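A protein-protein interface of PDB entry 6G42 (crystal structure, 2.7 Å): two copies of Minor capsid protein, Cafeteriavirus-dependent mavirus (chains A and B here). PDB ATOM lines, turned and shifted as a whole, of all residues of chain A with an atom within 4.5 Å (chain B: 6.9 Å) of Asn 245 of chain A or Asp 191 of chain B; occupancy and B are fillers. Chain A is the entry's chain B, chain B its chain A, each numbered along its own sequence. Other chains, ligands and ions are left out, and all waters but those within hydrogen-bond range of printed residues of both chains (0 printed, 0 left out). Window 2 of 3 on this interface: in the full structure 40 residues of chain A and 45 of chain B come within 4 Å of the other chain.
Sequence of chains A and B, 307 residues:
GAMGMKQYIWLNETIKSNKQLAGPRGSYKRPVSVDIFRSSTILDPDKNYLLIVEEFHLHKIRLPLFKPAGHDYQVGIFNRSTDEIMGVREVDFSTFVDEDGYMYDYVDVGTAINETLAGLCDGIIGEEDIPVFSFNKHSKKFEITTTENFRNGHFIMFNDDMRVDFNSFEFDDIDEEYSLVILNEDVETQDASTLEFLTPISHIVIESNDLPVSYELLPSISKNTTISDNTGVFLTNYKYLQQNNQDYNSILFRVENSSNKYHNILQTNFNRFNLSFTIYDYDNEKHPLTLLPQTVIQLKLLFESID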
ATOM      1  N   LEU A  65     -27.102  27.682 -20.119  1.00  0.00           N
ATOM      2  CA  LEU A  65     -28.196  27.735 -19.152  1.00  0.00           C
ATOM      3  C   LEU A  65     -28.659  29.155 -18.795  1.00  0.00           C
ATOM      4  O   LEU A  65     -29.704  29.323 -18.148  1.00  0.00           O
ATOM      5  CB  LEU A  65     -27.772  27.001 -17.872  1.00  0.00           C
ATOM      6  CG  LEU A  65     -27.163  25.599 -18.019  1.00  0.00           C
ATOM      7  CD1 LEU A  65     -27.065  24.933 -16.652  1.00  0.00           C
ATOM      8  CD2 LEU A  65     -27.949  24.710 -18.972  1.00  0.00           C
ATOM      9  N   ASP A 105     -23.740  27.058 -15.697  1.00  0.00           N
ATOM     10  CA  ASP A 105     -24.024  26.435 -14.398  1.00  0.00           C
ATOM     11  C   ASP A 105     -24.878  27.416 -13.575  1.00  0.00           C
ATOM     12  O   ASP A 105     -24.562  28.602 -13.530  1.00  0.00           O
ATOM     13  CB  ASP A 105     -22.698  26.110 -13.683  1.00  0.00           C
ATOM     14  CG  ASP A 105     -22.857  25.123 -12.513  1.00  0.00           C
ATOM     15  OD1 ASP A 105     -23.862  25.205 -11.761  1.00  0.00           O
ATOM     16  OD2 ASP A 105     -21.956  24.265 -12.335  1.00  0.00           O
ATOM     17  N   TYR A 106     -25.958  26.929 -12.951  1.00  0.00           N
ATOM     18  CA  TYR A 106     -26.821  27.780 -12.092  1.00  0.00           C
ATOM     19  C   TYR A 106     -26.217  28.032 -10.717  1.00  0.00           C
ATOM     20  O   TYR A 106     -26.712  28.883  -9.976  1.00  0.00           O
ATOM     21  CB  TYR A 106     -28.256  27.224 -11.941  1.00  0.00           C
ATOM     22  CG  TYR A 106     -29.050  27.275 -13.224  1.00  0.00           C
ATOM     23  CD1 TYR A 106     -29.317  28.492 -13.859  1.00  0.00           C
ATOM     24  CD2 TYR A 106     -29.518  26.107 -13.824  1.00  0.00           C
ATOM     25  CE1 TYR A 106     -30.028  28.541 -15.052  1.00  0.00           C
ATOM     26  CE2 TYR A 106     -30.233  26.147 -15.015  1.00  0.00           C
ATOM     27  CZ  TYR A 106     -30.486  27.362 -15.623  1.00  0.00           C
ATOM     28  OH  TYR A 106     -31.178  27.380 -16.807  1.00  0.00           O
ATOM     29  N   VAL A 107     -25.167  27.291 -10.369  1.00  0.00           N
ATOM     30  CA  VAL A 107     -24.350  27.622  -9.200  1.00  0.00           C
ATOM     31  C   VAL A 107     -23.701  28.993  -9.426  1.00  0.00           C
ATOM     32  O   VAL A 107     -23.791  29.868  -8.567  1.00  0.00           O
ATOM     33  CB  VAL A 107     -23.279  26.547  -8.904  1.00  0.00           C
ATOM     34  CG1 VAL A 107     -22.356  26.987  -7.771  1.00  0.00           C
ATOM     35  CG2 VAL A 107     -23.939  25.225  -8.538  1.00  0.00           C
ATOM     36  N   PHE A 135     -27.535  28.330  -4.941  1.00  0.00           N
ATOM     37  CA  PHE A 135     -28.306  27.361  -5.708  1.00  0.00           C
ATOM     38  C   PHE A 135     -28.098  25.982  -5.097  1.00  0.00           C
ATOM     39  O   PHE A 135     -26.966  25.539  -4.930  1.00  0.00           O
ATOM     40  CB  PHE A 135     -27.840  27.354  -7.169  1.00  0.00           C
ATOM     41  CG  PHE A 135     -28.556  26.350  -8.037  1.00  0.00           C
ATOM     42  CD1 PHE A 135     -29.888  26.543  -8.395  1.00  0.00           C
ATOM     43  CD2 PHE A 135     -27.899  25.214  -8.502  1.00  0.00           C
ATOM     44  CE1 PHE A 135     -30.551  25.622  -9.192  1.00  0.00           C
ATOM     45  CE2 PHE A 135     -28.559  24.289  -9.305  1.00  0.00           C
ATOM     46  CZ  PHE A 135     -29.886  24.495  -9.651  1.00  0.00           C
ATOM     47  N   LYS A 137     -28.029  22.174  -5.603  1.00  0.00           N
ATOM     48  CA  LYS A 137     -27.887  21.161  -6.664  1.00  0.00           C
ATOM     49  C   LYS A 137     -28.940  20.057  -6.551  1.00  0.00           C
ATOM     50  O   LYS A 137     -29.429  19.553  -7.560  1.00  0.00           O
ATOM     51  CB  LYS A 137     -26.520  20.479  -6.610  1.00  0.00           C
ATOM     52  CG  LYS A 137     -25.301  21.356  -6.823  1.00  0.00           C
ATOM     53  CD  LYS A 137     -24.059  20.481  -7.015  1.00  0.00           C
ATOM     54  CE  LYS A 137     -22.802  21.055  -6.371  1.00  0.00           C
ATOM     55  NZ  LYS A 137     -22.464  22.450  -6.781  1.00  0.00           N
ATOM     56  N   ASN A 244     -32.951  20.587 -15.531  1.00  0.00           N
ATOM     57  CA  ASN A 244     -31.993  20.489 -14.427  1.00  0.00           C
ATOM     58  C   ASN A 244     -30.775  21.404 -14.668  1.00  0.00           C
ATOM     59  O   ASN A 244     -30.863  22.361 -15.440  1.00  0.00           O
ATOM     60  CB  ASN A 244     -31.612  19.011 -14.244  1.00  0.00           C
ATOM     61  CG  ASN A 244     -30.944  18.415 -15.470  1.00  0.00           C
ATOM     62  OD1 ASN A 244     -30.767  19.077 -16.487  1.00  0.00           O
ATOM     63  ND2 ASN A 244     -30.576  17.146 -15.376  1.00  0.00           N
ATOM     64  N   ASN A 245     -29.650  21.112 -14.012  1.00  0.00           N
ATOM     65  CA  ASN A 245     -28.438  21.928 -14.105  1.00  0.00           C
ATOM     66  C   ASN A 245     -27.385  21.328 -15.050  1.00  0.00           C
ATOM     67  O   ASN A 245     -26.180  21.517 -14.861  1.00  0.00           O
ATOM     68  CB  ASN A 245     -27.857  22.097 -12.699  1.00  0.00           C
ATOM     69  CG  ASN A 245     -26.764  23.145 -12.637  1.00  0.00           C
ATOM     70  OD1 ASN A 245     -26.835  24.177 -13.314  1.00  0.00           O
ATOM     71  ND2 ASN A 245     -25.737  22.883 -11.830  1.00  0.00           N
ATOM     72  N   GLN A 246     -27.839  20.618 -16.076  1.00  0.00           N
ATOM     73  CA  GLN A 246     -26.937  19.916 -16.978  1.00  0.00           C
ATOM     74  C   GLN A 246     -26.708  20.722 -18.252  1.00  0.00           C
ATOM     75  O   GLN A 246     -27.608  20.858 -19.089  1.00  0.00           O
ATOM     76  CB  GLN A 246     -27.497  18.545 -17.326  1.00  0.00           C
ATOM     77  CG  GLN A 246     -27.315  17.487 -16.252  1.00  0.00           C
ATOM     78  CD  GLN A 246     -27.583  16.097 -16.806  1.00  0.00           C
ATOM     79  OE1 GLN A 246     -28.738  15.711 -17.002  1.00  0.00           O
ATOM     80  NE2 GLN A 246     -26.520  15.352 -17.093  1.00  0.00           N
ATOM     81  N   ASP A 247     -25.504  21.265 -18.382  1.00  0.00           N
ATOM     82  CA  ASP A 247     -25.073  21.914 -19.622  1.00  0.00           C
ATOM     83  C   ASP A 247     -24.825  20.887 -20.736  1.00  0.00           C
ATOM     84  O   ASP A 247     -25.115  21.153 -21.905  1.00  0.00           O
ATOM     85  CB  ASP A 247     -23.856  22.846 -19.409  1.00  0.00           C
ATOM     86  CG  ASP A 247     -22.743  22.225 -18.565  1.00  0.00           C
ATOM     87  OD1 ASP A 247     -22.979  21.185 -17.914  1.00  0.00           O
ATOM     88  OD2 ASP A 247     -21.627  22.798 -18.540  1.00  0.00           O
ATOM     89  N   LYS B 141     -25.933   6.867  -9.574  1.00  0.00           N
ATOM     90  CA  LYS B 141     -25.000   7.981  -9.716  1.00  0.00           C
ATOM     91  C   LYS B 141     -23.635   7.552  -9.201  1.00  0.00           C
ATOM     92  O   LYS B 141     -23.532   6.837  -8.200  1.00  0.00           O
ATOM     93  CB  LYS B 141     -25.482   9.186  -8.915  1.00  0.00           C
ATOM     94  CG  LYS B 141     -26.716   9.864  -9.481  1.00  0.00           C
ATOM     95  CD  LYS B 141     -27.366  10.788  -8.462  1.00  0.00           C
ATOM     96  CE  LYS B 141     -28.452  11.628  -9.117  1.00  0.00           C
ATOM     97  NZ  LYS B 141     -29.081  12.594  -8.182  1.00  0.00           N
ATOM     98  N   PHE B 142     -22.584   7.998  -9.878  1.00  0.00           N
ATOM     99  CA  PHE B 142     -21.229   7.752  -9.411  1.00  0.00           C
ATOM    100  C   PHE B 142     -20.886   8.707  -8.260  1.00  0.00           C
ATOM    101  O   PHE B 142     -21.437   9.813  -8.170  1.00  0.00           O
ATOM    102  CB  PHE B 142     -20.239   7.876 -10.564  1.00  0.00           C
ATOM    103  CG  PHE B 142     -20.369   6.779 -11.587  1.00  0.00           C
ATOM    104  CD1 PHE B 142     -21.282   6.887 -12.635  1.00  0.00           C
ATOM    105  CD2 PHE B 142     -19.580   5.637 -11.506  1.00  0.00           C
ATOM    106  CE1 PHE B 142     -21.403   5.879 -13.583  1.00  0.00           C
ATOM    107  CE2 PHE B 142     -19.697   4.625 -12.450  1.00  0.00           C
ATOM    108  CZ  PHE B 142     -20.609   4.748 -13.491  1.00  0.00           C
ATOM    109  N   ASN B 167     -20.455  14.330 -16.531  1.00  0.00           N
ATOM    110  CA  ASN B 167     -20.634  15.796 -16.575  1.00  0.00           C
ATOM    111  C   ASN B 167     -21.358  16.431 -15.398  1.00  0.00           C
ATOM    112  O   ASN B 167     -21.288  17.645 -15.220  1.00  0.00           O
ATOM    113  CB  ASN B 167     -21.329  16.222 -17.889  1.00  0.00           C
ATOM    114  CG  ASN B 167     -22.708  15.586 -18.075  1.00  0.00           C
ATOM    115  OD1 ASN B 167     -23.687  16.016 -17.461  1.00  0.00           O
ATOM    116  ND2 ASN B 167     -22.794  14.580 -18.941  1.00  0.00           N
ATOM    117  N   SER B 168     -22.055  15.621 -14.613  1.00  0.00           N
ATOM    118  CA  SER B 168     -22.823  16.102 -13.468  1.00  0.00           C
ATOM    119  C   SER B 168     -22.012  16.554 -12.248  1.00  0.00           C
ATOM    120  O   SER B 168     -22.553  17.242 -11.374  1.00  0.00           O
ATOM    121  CB  SER B 168     -23.773  15.009 -13.024  1.00  0.00           C
ATOM    122  OG  SER B 168     -24.602  14.597 -14.088  1.00  0.00           O
ATOM    123  N   PHE B 169     -20.744  16.155 -12.160  1.00  0.00           N
ATOM    124  CA  PHE B 169     -19.851  16.687 -11.123  1.00  0.00           C
ATOM    125  C   PHE B 169     -19.595  18.177 -11.394  1.00  0.00           C
ATOM    126  O   PHE B 169     -19.828  18.661 -12.509  1.00  0.00           O
ATOM    127  CB  PHE B 169     -18.515  15.939 -11.095  1.00  0.00           C
ATOM    128  CG  PHE B 169     -18.595  14.532 -10.551  1.00  0.00           C
ATOM    129  CD1 PHE B 169     -18.860  14.303  -9.205  1.00  0.00           C
ATOM    130  CD2 PHE B 169     -18.357  13.428 -11.381  1.00  0.00           C
ATOM    131  CE1 PHE B 169     -18.911  13.006  -8.706  1.00  0.00           C
ATOM    132  CE2 PHE B 169     -18.404  12.131 -10.883  1.00  0.00           C
ATOM    133  CZ  PHE B 169     -18.681  11.920  -9.543  1.00  0.00           C
ATOM    134  N   GLU B 170     -19.134  18.894 -10.370  1.00  0.00           N
ATOM    135  CA  GLU B 170     -18.715  20.292 -10.532  1.00  0.00           C
ATOM    136  C   GLU B 170     -17.264  20.309 -11.003  1.00  0.00           C
ATOM    137  O   GLU B 170     -16.412  19.667 -10.392  1.00  0.00           O
ATOM    138  CB  GLU B 170     -18.870  21.080  -9.224  1.00  0.00           C
ATOM    139  CG  GLU B 170     -18.690  22.591  -9.384  1.00  0.00           C
ATOM    140  CD  GLU B 170     -18.866  23.378  -8.090  1.00  0.00           C
ATOM    141  OE1 GLU B 170     -19.207  22.782  -7.040  1.00  0.00           O
ATOM    142  OE2 GLU B 170     -18.658  24.612  -8.127  1.00  0.00           O
ATOM    143  N   THR B 189     -21.360  13.349  -4.816  1.00  0.00           N
ATOM    144  CA  THR B 189     -22.095  12.601  -5.841  1.00  0.00           C
ATOM    145  C   THR B 189     -22.397  13.483  -7.052  1.00  0.00           C
ATOM    146  O   THR B 189     -22.239  14.704  -7.008  1.00  0.00           O
ATOM    147  CB  THR B 189     -23.411  11.998  -5.281  1.00  0.00           C
ATOM    148  OG1 THR B 189     -24.089  11.269  -6.312  1.00  0.00           O
ATOM    149  CG2 THR B 189     -24.354  13.074  -4.737  1.00  0.00           C
ATOM    150  N   GLN B 190     -22.822  12.845  -8.134  1.00  0.00           N
ATOM    151  CA  GLN B 190     -23.313  13.549  -9.311  1.00  0.00           C
ATOM    152  C   GLN B 190     -24.646  14.231  -8.991  1.00  0.00           C
ATOM    153  O   GLN B 190     -25.470  13.675  -8.262  1.00  0.00           O
ATOM    154  CB  GLN B 190     -23.519  12.553 -10.448  1.00  0.00           C
ATOM    155  CG  GLN B 190     -22.243  12.071 -11.112  1.00  0.00           C
ATOM    156  CD  GLN B 190     -22.513  11.032 -12.191  1.00  0.00           C
ATOM    157  OE1 GLN B 190     -22.820   9.885 -11.887  1.00  0.00           O
ATOM    158  NE2 GLN B 190     -22.393  11.429 -13.456  1.00  0.00           N
ATOM    159  N   ASP B 191     -24.857  15.429  -9.538  1.00  0.00           N
ATOM    160  CA  ASP B 191     -26.153  16.121  -9.397  1.00  0.00           C
ATOM    161  C   ASP B 191     -27.265  15.522 -10.300  1.00  0.00           C
ATOM    162  O   ASP B 191     -28.446  15.815 -10.107  1.00  0.00           O
ATOM    163  CB  ASP B 191     -26.002  17.668  -9.511  1.00  0.00           C
ATOM    164  CG  ASP B 191     -25.945  18.207 -10.960  1.00  0.00           C
ATOM    165  OD1 ASP B 191     -25.952  17.440 -11.942  1.00  0.00           O
ATOM    166  OD2 ASP B 191     -25.896  19.450 -11.113  1.00  0.00           O
ATOM    167  N   ALA B 192     -26.872  14.670 -11.249  1.00  0.00           N
ATOM    168  CA  ALA B 192     -27.776  14.035 -12.206  1.00  0.00           C
ATOM    169  C   ALA B 192     -27.147  12.749 -12.727  1.00  0.00           C
ATOM    170  O   ALA B 192     -25.924  12.623 -12.784  1.00  0.00           O
ATOM    171  CB  ALA B 192     -28.077  14.972 -13.364  1.00  0.00           C
ATOM    172  N   SER B 193     -27.995  11.799 -13.114  1.00  0.00           N
ATOM    173  CA  SER B 193     -27.543  10.516 -13.656  1.00  0.00           C
ATOM    174  C   SER B 193     -26.998  10.709 -15.077  1.00  0.00           C
ATOM    175  O   SER B 193     -27.505  11.543 -15.836  1.00  0.00           O
ATOM    176  CB  SER B 193     -28.695   9.513 -13.648  1.00  0.00           C
ATOM    177  OG  SER B 193     -28.213   8.186 -13.676  1.00  0.00           O
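Of the 10 printed residues of chain A, 4 touch a printed residue of chain B. Hydrophobic or aromatic side chains of chain B within 4 Å of the printed part of chain A: Ala 192. Among the printed residues, Asp or Glu carboxylates within 4 Å of a Lys or Arg side-chain nitrogen of the other chain: Lys 137 of chain A with Glu 170 of chain B.
The side-chain hydroxyl of Ser 168 of chain B lies within hydrogen-bond range of the backbone carbonyl oxygen of Ala 192 of chain B. The side-chain amide nitrogen of Asn 244 of chain A is in hydrogen-bond range of the side-chain amide oxygen of Gln 246 of chain A. The backbone NH of Tyr 106 of chain A lies within hydrogen-bond range of the side-chain amide oxygen of Asn 245 of chain A, at 2.9 Å. The backbone carbonyl oxygen (O) of Ser 168 of chain B sits at hydrogen-bond distance from the backbone NH (N) of Asp 191 of chain B (3.5 Å). OD1 of Asp 105 of chain A is in hydrogen-bond range of ND2 of Asn 245 of chain A, 3.0 Å away.
Printed residues of chain B within 4 Å of Lys 137 of chain A: Glu 170. Of the printed residues of chain B, Asn 244 of chain A touches Ala 192 (3.9 Å). Of the printed residues of chain A, Ser 168 of chain B touches Gln 246 (3.6 Å). Of the printed residues of chain A, Glu 170 of chain B touches Lys 137 (3.3 Å). Thr 189 of chain B touches none of the printed residues of chain A. Gln 190 of chain B touches none of the printed residues of chain A.
CB of Ala 192 of chain B touches ND2 of Asn 244 of chain A (3.9 Å). OD2 of Asp 191 of chain B touches ND2 of Asn 245 of chain A (3.5 Å). Ser 168 of chain B touches Gln 246 of chain A. Ala 192 of chain B touches Gln 246 of chain A.
NE2 of Gln 246 of chain A sits at hydrogen-bond distance from OD1 of Asn 167 of chain B (2.9 Å). The side-chain carboxylate of Glu 170 of chain B lies within salt-bridge range of the side-chain amino group of Lys 137 of chain A, 3.3 Å away.
No position is printed for both chains. Of the 6 pairs that touch across the chains among the printed residues, none has its exchanged pair printed and touching as well.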
